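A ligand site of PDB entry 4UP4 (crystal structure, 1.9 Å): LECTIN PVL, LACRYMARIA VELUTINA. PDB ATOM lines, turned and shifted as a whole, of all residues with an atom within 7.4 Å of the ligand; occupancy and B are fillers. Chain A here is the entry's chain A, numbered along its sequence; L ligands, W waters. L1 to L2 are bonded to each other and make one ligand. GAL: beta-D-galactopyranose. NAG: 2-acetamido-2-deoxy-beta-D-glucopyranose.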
ATOM      1  N   ASN A  45     -25.039 -19.981  -7.082  1.00  0.00           N
ATOM      2  CA  ASN A  45     -23.647 -20.310  -7.371  1.00  0.00           C
ATOM      3  C   ASN A  45     -22.868 -20.398  -6.068  1.00  0.00           C
ATOM      4  O   ASN A  45     -21.919 -19.632  -5.812  1.00  0.00           O
ATOM      5  CB  ASN A  45     -23.069 -19.269  -8.330  1.00  0.00           C
ATOM      6  CG  ASN A  45     -21.731 -19.671  -8.862  1.00  0.00           C
ATOM      7  OD1 ASN A  45     -21.508 -20.846  -9.177  1.00  0.00           O
ATOM      8  ND2 ASN A  45     -20.793 -18.726  -8.908  1.00  0.00           N
ATOM      9  N   ASN A  46     -23.316 -21.311  -5.223  1.00  0.00           N
ATOM     10  CA  ASN A  46     -22.807 -21.510  -3.862  1.00  0.00           C
ATOM     11  C   ASN A  46     -23.334 -22.855  -3.312  1.00  0.00           C
ATOM     12  O   ASN A  46     -24.078 -23.525  -4.002  1.00  0.00           O
ATOM     13  CB  ASN A  46     -23.192 -20.324  -2.967  1.00  0.00           C
ATOM     14  CG  ASN A  46     -22.097 -19.917  -2.005  1.00  0.00           C
ATOM     15  OD1 ASN A  46     -21.578 -20.725  -1.239  1.00  0.00           O
ATOM     16  ND2 ASN A  46     -21.738 -18.655  -2.040  1.00  0.00           N
ATOM     17  N   PHE A  47     -22.905 -23.236  -2.100  1.00  0.00           N
ATOM     18  CA  PHE A  47     -23.258 -24.515  -1.444  1.00  0.00           C
ATOM     19  C   PHE A  47     -22.819 -25.713  -2.262  1.00  0.00           C
ATOM     20  O   PHE A  47     -23.475 -26.764  -2.245  1.00  0.00           O
ATOM     21  CB  PHE A  47     -24.752 -24.616  -1.138  1.00  0.00           C
ATOM     22  CG  PHE A  47     -25.266 -23.466  -0.310  1.00  0.00           C
ATOM     23  CD1 PHE A  47     -25.021 -23.427   1.042  1.00  0.00           C
ATOM     24  CD2 PHE A  47     -25.959 -22.428  -0.885  1.00  0.00           C
ATOM     25  CE1 PHE A  47     -25.506 -22.370   1.814  1.00  0.00           C
ATOM     26  CE2 PHE A  47     -26.415 -21.369  -0.156  1.00  0.00           C
ATOM     27  CZ  PHE A  47     -26.170 -21.330   1.196  1.00  0.00           C
ATOM     28  N   GLY A  48     -21.772 -25.537  -3.041  1.00  0.00           N
ATOM     29  CA  GLY A  48     -21.310 -26.571  -3.966  1.00  0.00           C
ATOM     30  C   GLY A  48     -19.871 -26.986  -3.674  1.00  0.00           C
ATOM     31  O   GLY A  48     -19.116 -26.235  -3.049  1.00  0.00           O
ATOM     32  N   ALA A  51     -18.234 -24.542  -5.715  1.00  0.00           N
ATOM     33  CA  ALA A  51     -18.798 -23.222  -5.527  1.00  0.00           C
ATOM     34  C   ALA A  51     -18.943 -22.968  -4.045  1.00  0.00           C
ATOM     35  O   ALA A  51     -19.989 -23.236  -3.445  1.00  0.00           O
ATOM     36  CB  ALA A  51     -20.117 -23.146  -6.232  1.00  0.00           C
ATOM     37  N   GLY A  52     -17.844 -22.542  -3.427  1.00  0.00           N
ATOM     38  CA  GLY A  52     -17.831 -22.394  -2.006  1.00  0.00           C
ATOM     39  C   GLY A  52     -17.058 -23.395  -1.188  1.00  0.00           C
ATOM     40  O   GLY A  52     -16.954 -23.240   0.043  1.00  0.00           O
ATOM     41  N   GLY A  53     -16.487 -24.411  -1.831  1.00  0.00           N
ATOM     42  CA  GLY A  53     -15.713 -25.390  -1.073  1.00  0.00           C
ATOM     43  C   GLY A  53     -16.491 -26.267  -0.084  1.00  0.00           C
ATOM     44  O   GLY A  53     -15.953 -26.678   0.977  1.00  0.00           O
ATOM     45  N   TRP A  54     -17.736 -26.586  -0.453  1.00  0.00           N
ATOM     46  CA  TRP A  54     -18.579 -27.404   0.414  1.00  0.00           C
ATOM     47  C   TRP A  54     -18.187 -28.890   0.296  1.00  0.00           C
ATOM     48  O   TRP A  54     -17.936 -29.416  -0.806  1.00  0.00           O
ATOM     49  CB  TRP A  54     -20.056 -27.153   0.122  1.00  0.00           C
ATOM     50  CG  TRP A  54     -20.434 -25.791   0.560  1.00  0.00           C
ATOM     51  CD1 TRP A  54     -20.136 -24.629  -0.084  1.00  0.00           C
ATOM     52  CD2 TRP A  54     -21.196 -25.407   1.730  1.00  0.00           C
ATOM     53  NE1 TRP A  54     -20.629 -23.556   0.607  1.00  0.00           N
ATOM     54  CE2 TRP A  54     -21.282 -23.993   1.721  1.00  0.00           C
ATOM     55  CE3 TRP A  54     -21.830 -26.110   2.764  1.00  0.00           C
ATOM     56  CZ2 TRP A  54     -21.942 -23.270   2.696  1.00  0.00           C
ATOM     57  CZ3 TRP A  54     -22.447 -25.396   3.753  1.00  0.00           C
ATOM     58  CH2 TRP A  54     -22.502 -23.994   3.729  1.00  0.00           C
ATOM     59  N   ARG A  55     -18.094 -29.539   1.455  1.00  0.00           N
ATOM     60  CA  ARG A  55     -17.645 -30.892   1.612  1.00  0.00           C
ATOM     61  C   ARG A  55     -18.654 -31.701   2.452  1.00  0.00           C
ATOM     62  O   ARG A  55     -19.061 -31.304   3.553  1.00  0.00           O
ATOM     63  CB  ARG A  55     -16.302 -30.921   2.281  1.00  0.00           C
ATOM     64  CG  ARG A  55     -15.196 -30.213   1.492  1.00  0.00           C
ATOM     65  CD  ARG A  55     -14.864 -31.023   0.224  1.00  0.00           C
ATOM     66  NE  ARG A  55     -13.782 -30.390  -0.482  1.00  0.00           N
ATOM     67  CZ  ARG A  55     -13.950 -29.405  -1.357  1.00  0.00           C
ATOM     68  NH1 ARG A  55     -15.180 -28.927  -1.658  1.00  0.00           N
ATOM     69  NH2 ARG A  55     -12.879 -28.875  -1.916  1.00  0.00           N
ATOM     70  N   LYS A  58     -17.544 -32.357   6.071  1.00  0.00           N
ATOM     71  CA  LYS A  58     -17.415 -31.234   6.991  1.00  0.00           C
ATOM     72  C   LYS A  58     -18.584 -30.353   7.152  1.00  0.00           C
ATOM     73  O   LYS A  58     -18.648 -29.640   8.140  1.00  0.00           O
ATOM     74  CB  LYS A  58     -16.226 -30.328   6.548  1.00  0.00           C
ATOM     75  CG  LYS A  58     -14.885 -31.048   6.484  1.00  0.00           C
ATOM     76  CD  LYS A  58     -13.759 -30.081   6.141  1.00  0.00           C
ATOM     77  CE  LYS A  58     -13.652 -28.904   7.078  1.00  0.00           C
ATOM     78  NZ  LYS A  58     -12.433 -28.116   6.738  1.00  0.00           N
ATOM     79  N   HIS A  59     -19.490 -30.306   6.150  1.00  0.00           N
ATOM     80  CA  HIS A  59     -20.570 -29.324   6.112  1.00  0.00           C
ATOM     81  C   HIS A  59     -21.928 -30.021   5.929  1.00  0.00           C
ATOM     82  O   HIS A  59     -21.982 -31.195   5.513  1.00  0.00           O
ATOM     83  CB  HIS A  59     -20.298 -28.360   5.001  1.00  0.00           C
ATOM     84  CG  HIS A  59     -18.936 -27.784   5.060  1.00  0.00           C
ATOM     85  ND1 HIS A  59     -18.067 -27.799   3.985  1.00  0.00           N
ATOM     86  CD2 HIS A  59     -18.257 -27.226   6.082  1.00  0.00           C
ATOM     87  CE1 HIS A  59     -16.915 -27.247   4.348  1.00  0.00           C
ATOM     88  NE2 HIS A  59     -16.998 -26.943   5.624  1.00  0.00           N
ATOM     89  N   GLY A  76     -27.030 -23.906   4.862  1.00  0.00           N
ATOM     90  CA  GLY A  76     -25.806 -24.660   4.941  1.00  0.00           C
ATOM     91  C   GLY A  76     -25.011 -24.310   6.172  1.00  0.00           C
ATOM     92  O   GLY A  76     -24.761 -23.130   6.462  1.00  0.00           O
ATOM     93  N   PHE A  77     -24.675 -25.356   6.919  1.00  0.00           N
ATOM     94  CA  PHE A  77     -23.745 -25.313   8.012  1.00  0.00           C
ATOM     95  C   PHE A  77     -22.337 -25.460   7.467  1.00  0.00           C
ATOM     96  O   PHE A  77     -21.870 -26.560   7.180  1.00  0.00           O
ATOM     97  CB  PHE A  77     -24.059 -26.442   8.988  1.00  0.00           C
ATOM     98  CG  PHE A  77     -25.436 -26.350   9.592  1.00  0.00           C
ATOM     99  CD1 PHE A  77     -26.559 -26.925   8.962  1.00  0.00           C
ATOM    100  CD2 PHE A  77     -25.626 -25.746  10.823  1.00  0.00           C
ATOM    101  CE1 PHE A  77     -27.827 -26.824   9.528  1.00  0.00           C
ATOM    102  CE2 PHE A  77     -26.895 -25.711  11.412  1.00  0.00           C
ATOM    103  CZ  PHE A  77     -27.986 -26.212  10.752  1.00  0.00           C
ATOM    104  N   GLY A  78     -21.680 -24.335   7.274  1.00  0.00           N
ATOM    105  CA  GLY A  78     -20.434 -24.322   6.554  1.00  0.00           C
ATOM    106  C   GLY A  78     -19.223 -24.346   7.441  1.00  0.00           C
ATOM    107  O   GLY A  78     -19.210 -24.930   8.496  1.00  0.00           O
ATOM    108  N   GLU A  79     -18.155 -23.674   7.013  1.00  0.00           N
ATOM    109  CA  GLU A  79     -16.863 -23.741   7.743  1.00  0.00           C
ATOM    110  C   GLU A  79     -16.859 -22.882   8.973  1.00  0.00           C
ATOM    111  O   GLU A  79     -16.427 -23.315  10.031  1.00  0.00           O
ATOM    112  CB  GLU A  79     -15.706 -23.316   6.845  1.00  0.00           C
ATOM    113  CG  GLU A  79     -14.314 -23.649   7.374  1.00  0.00           C
ATOM    114  CD  GLU A  79     -13.987 -25.135   7.303  1.00  0.00           C
ATOM    115  OE1 GLU A  79     -14.838 -25.976   6.871  1.00  0.00           O
ATOM    116  OE2 GLU A  79     -12.909 -25.514   7.773  1.00  0.00           O
ATOM    117  N   ASN A  80     -17.298 -21.631   8.844  1.00  0.00           N
ATOM    118  CA  ASN A  80     -17.271 -20.650   9.930  1.00  0.00           C
ATOM    119  C   ASN A  80     -18.593 -20.104  10.385  1.00  0.00           C
ATOM    120  O   ASN A  80     -18.647 -19.209  11.155  1.00  0.00           O
ATOM    121  CB  ASN A  80     -16.341 -19.485   9.540  1.00  0.00           C
ATOM    122  CG  ASN A  80     -14.937 -19.972   9.470  1.00  0.00           C
ATOM    123  OD1 ASN A  80     -14.379 -20.241  10.484  1.00  0.00           O
ATOM    124  ND2 ASN A  80     -14.432 -20.241   8.289  1.00  0.00           N
ATOM    125  N   GLY A  81     -19.667 -20.717   9.937  1.00  0.00           N
ATOM    126  CA  GLY A  81     -20.980 -20.314  10.382  1.00  0.00           C
ATOM    127  C   GLY A  81     -22.067 -20.909   9.552  1.00  0.00           C
ATOM    128  O   GLY A  81     -21.819 -21.779   8.641  1.00  0.00           O
ATOM    129  N   VAL A  82     -23.272 -20.431   9.816  1.00  0.00           N
ATOM    130  CA  VAL A  82     -24.466 -20.909   9.123  1.00  0.00           C
ATOM    131  C   VAL A  82     -24.812 -19.896   8.042  1.00  0.00           C
ATOM    132  O   VAL A  82     -24.975 -18.693   8.322  1.00  0.00           O
ATOM    133  CB  VAL A  82     -25.653 -21.092  10.086  1.00  0.00           C
ATOM    134  CG1 VAL A  82     -26.939 -21.475   9.360  1.00  0.00           C
ATOM    135  CG2 VAL A  82     -25.312 -22.145  11.121  1.00  0.00           C
ATOM    136  N   TRP A  83     -24.947 -20.387   6.824  1.00  0.00           N
ATOM    137  CA  TRP A  83     -25.235 -19.571   5.650  1.00  0.00           C
ATOM    138  C   TRP A  83     -26.635 -19.846   5.049  1.00  0.00           C
ATOM    139  O   TRP A  83     -26.974 -21.004   4.833  1.00  0.00           O
ATOM    140  CB  TRP A  83     -24.220 -19.843   4.585  1.00  0.00           C
ATOM    141  CG  TRP A  83     -22.845 -19.417   4.923  1.00  0.00           C
ATOM    142  CD1 TRP A  83     -21.908 -20.134   5.570  1.00  0.00           C
ATOM    143  CD2 TRP A  83     -22.215 -18.177   4.545  1.00  0.00           C
ATOM    144  NE1 TRP A  83     -20.731 -19.422   5.633  1.00  0.00           N
ATOM    145  CE2 TRP A  83     -20.900 -18.224   4.993  1.00  0.00           C
ATOM    146  CE3 TRP A  83     -22.653 -17.021   3.841  1.00  0.00           C
ATOM    147  CZ2 TRP A  83     -19.993 -17.149   4.803  1.00  0.00           C
ATOM    148  CZ3 TRP A  83     -21.738 -15.941   3.650  1.00  0.00           C
ATOM    149  CH2 TRP A  83     -20.444 -16.023   4.137  1.00  0.00           C
ATOM    150  N   PRO A  96     -25.442 -13.806  -3.265  1.00  0.00           N
ATOM    151  CA  PRO A  96     -24.953 -14.843  -2.402  1.00  0.00           C
ATOM    152  C   PRO A  96     -25.798 -15.069  -1.152  1.00  0.00           C
ATOM    153  O   PRO A  96     -26.589 -14.186  -0.747  1.00  0.00           O
ATOM    154  CB  PRO A  96     -23.537 -14.338  -2.005  1.00  0.00           C
ATOM    155  CG  PRO A  96     -23.666 -12.851  -2.073  1.00  0.00           C
ATOM    156  CD  PRO A  96     -24.571 -12.616  -3.243  1.00  0.00           C
ATOM    157  N   PRO A  97     -25.577 -16.196  -0.493  1.00  0.00           N
ATOM    158  CA  PRO A  97     -26.144 -16.379   0.805  1.00  0.00           C
ATOM    159  C   PRO A  97     -25.585 -15.446   1.860  1.00  0.00           C
ATOM    160  O   PRO A  97     -24.485 -14.913   1.730  1.00  0.00           O
ATOM    161  CB  PRO A  97     -25.767 -17.805   1.153  1.00  0.00           C
ATOM    162  CG  PRO A  97     -24.483 -18.019   0.416  1.00  0.00           C
ATOM    163  CD  PRO A  97     -24.666 -17.295  -0.874  1.00  0.00           C
ATOM    164  N   MET A  99     -24.428 -14.969   6.006  1.00  0.00           N
ATOM    165  CA  MET A  99     -23.955 -15.636   7.222  1.00  0.00           C
ATOM    166  C   MET A  99     -24.757 -15.123   8.464  1.00  0.00           C
ATOM    167  O   MET A  99     -24.541 -14.019   8.942  1.00  0.00           O
ATOM    168  CB  MET A  99     -22.442 -15.388   7.355  1.00  0.00           C
ATOM    169  CG  MET A  99     -21.726 -16.560   8.076  1.00  0.00           C
ATOM    170  SD  MET A  99     -22.159 -16.639   9.824  1.00  0.00           S
ATOM    171  CE  MET A  99     -21.325 -15.152  10.417  1.00  0.00           C
ATOM    172  N   ALA A 105     -20.751 -24.851  13.280  1.00  0.00           N
ATOM    173  CA  ALA A 105     -19.869 -24.969  12.151  1.00  0.00           C
ATOM    174  C   ALA A 105     -18.548 -25.648  12.514  1.00  0.00           C
ATOM    175  O   ALA A 105     -18.121 -25.726  13.668  1.00  0.00           O
ATOM    176  CB  ALA A 105     -19.607 -23.622  11.508  1.00  0.00           C
ATOM    177  N   ALA A 107     -15.427 -24.877  12.193  1.00  0.00           N
ATOM    178  CA  ALA A 107     -14.346 -24.099  12.788  1.00  0.00           C
ATOM    179  C   ALA A 107     -15.019 -22.995  13.646  1.00  0.00           C
ATOM    180  O   ALA A 107     -14.375 -22.081  14.146  1.00  0.00           O
ATOM    181  CB  ALA A 107     -13.439 -23.528  11.719  1.00  0.00           C
HETATM  182  C1  GAL L   1     -12.739 -20.562   4.576  1.00  0.00           C
HETATM  183  C2  GAL L   1     -14.214 -20.946   4.425  1.00  0.00           C
HETATM  184  C3  GAL L   1     -15.009 -19.809   3.844  1.00  0.00           C
HETATM  185  C4  GAL L   1     -14.932 -18.593   4.750  1.00  0.00           C
HETATM  186  C5  GAL L   1     -13.438 -18.330   5.087  1.00  0.00           C
HETATM  187  C6  GAL L   1     -13.238 -17.408   6.291  1.00  0.00           C
HETATM  188  O1  GAL L   1     -12.133 -21.614   5.246  1.00  0.00           O
HETATM  189  O2  GAL L   1     -14.255 -22.015   3.525  1.00  0.00           O
HETATM  190  O3  GAL L   1     -16.363 -20.220   3.751  1.00  0.00           O
HETATM  191  O4  GAL L   1     -15.827 -18.638   5.881  1.00  0.00           O
HETATM  192  O5  GAL L   1     -12.673 -19.470   5.419  1.00  0.00           O
HETATM  193  O6  GAL L   1     -11.917 -16.879   6.169  1.00  0.00           O
HETATM  194  C1  NAG L   2     -16.994 -19.768   2.549  1.00  0.00           C
HETATM  195  C2  NAG L   2     -18.341 -20.527   2.417  1.00  0.00           C
HETATM  196  C3  NAG L   2     -19.107 -20.041   1.175  1.00  0.00           C
HETATM  197  C4  NAG L   2     -19.175 -18.514   1.122  1.00  0.00           C
HETATM  198  C5  NAG L   2     -17.772 -17.932   1.349  1.00  0.00           C
HETATM  199  C6  NAG L   2     -17.812 -16.408   1.419  1.00  0.00           C
HETATM  200  C7  NAG L   2     -18.240 -22.775   3.446  1.00  0.00           C
HETATM  201  C8  NAG L   2     -18.052 -24.208   3.118  1.00  0.00           C
HETATM  202  N2  NAG L   2     -18.133 -21.968   2.394  1.00  0.00           N
HETATM  203  O3  NAG L   2     -20.414 -20.592   1.105  1.00  0.00           O
HETATM  204  O4  NAG L   2     -19.629 -18.069  -0.137  1.00  0.00           O
HETATM  205  O5  NAG L   2     -17.238 -18.378   2.578  1.00  0.00           O
HETATM  206  O6  NAG L   2     -16.481 -15.927   1.501  1.00  0.00           O
HETATM  207  O7  NAG L   2     -18.489 -22.403   4.616  1.00  0.00           O
HETATM  208  O   HOH W   1     -11.667 -21.066   8.297  1.00  0.00           O
HETATM  209  O   HOH W   2     -21.108 -15.531  -0.029  1.00  0.00           O
HETATM  210  O   HOH W   3     -18.447 -18.660  -2.276  1.00  0.00           O
HETATM  211  O   HOH W   4     -14.327 -22.107   1.000  1.00  0.00           O
HETATM  212  O   HOH W   5     -17.936 -20.324   6.233  1.00  0.00           O
HETATM  213  O   HOH W   6     -10.091 -18.721   4.905  1.00  0.00           O
HETATM  214  O   HOH W   7     -10.997 -24.665   5.460  1.00  0.00           O
HETATM  215  O   HOH W   8     -10.004 -16.481   8.583  1.00  0.00           O
HETATM  216  O   HOH W   9      -9.696 -15.400   4.600  1.00  0.00           O
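The side-chain amide oxygen of Asn 46 sits at hydrogen-bond distance from an oxygen (O3) of NAG L2, 2.6 Å away.
An oxygen (O7) of NAG L2 is in hydrogen-bond range of the backbone NH (N) of Glu 79, at 2.7 Å.
The backbone carbonyl oxygen of Gly 52 sits at hydrogen-bond distance from a nitrogen (N2) of NAG L2 (2.9 Å).
An oxygen (O3) of NAG L2 is in hydrogen-bond range of the indole nitrogen of Trp 54, 3.0 Å away.
O4 of GAL L1 lies within hydrogen-bond range of ND2 of Asn 80 (3.2 Å).
A ring nitrogen (NE2) of His 59 is in hydrogen-bond range of the side-chain carboxylate (OE1) of Glu 79, at 2.7 Å.
The side-chain carboxylate (OE2) of Glu 79 lies within salt-bridge range of the side-chain amino group (NZ) of Lys 58 (2.8 Å).
N of Ala 107 is in hydrogen-bond range of O of Glu 79 (2.8 Å).
The backbone NH of Trp 54 lies within hydrogen-bond range of the backbone carbonyl oxygen of Gly 48, 3.0 Å away.
ND1 of His 59 is in hydrogen-bond range of N of Arg 55.
The backbone carbonyl oxygen of Gly 76 is in hydrogen-bond range of the backbone NH of Trp 83 (2.8 Å).
The backbone NH (N) of Gly 53 is in hydrogen-bond range of the backbone carbonyl oxygen (O) of Gly 48, 3.4 Å away.
O of Gly 53 touches C8 of NAG L2, 3.9 Å away.
CE1 of His 59 touches C8 of NAG L2, 3.5 Å away.
CA of Gly 78 touches O7 of NAG L2, 3.3 Å away.
Trp 83 touches the ligand.
Hydrophobic or aromatic side chains that line the ligand: Trp 54, His 59 and Trp 83.
Of the 24 residues printed, 9 come within 4 Å of the ligand.
The nearest printed residue that does not touch the ligand is Phe 47 (4.8 Å).
Water W3 lies within hydrogen-bond range of O4 of NAG L2 and ND2 of Asn 46.
Water W4 lies within hydrogen-bond range of O2 of GAL L1 (2.5 Å) and O of Gly 52 (3.0 Å).
Water W1 bridges the side-chain amide nitrogen (ND2) of Asn 80 (2.9 Å) and an oxygen (O1) of GAL L1 (3.1 Å).
Water W7 bridges the side-chain carboxylate of Glu 79 (3.1 Å) and an oxygen (O1) of GAL L1 (3.3 Å).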
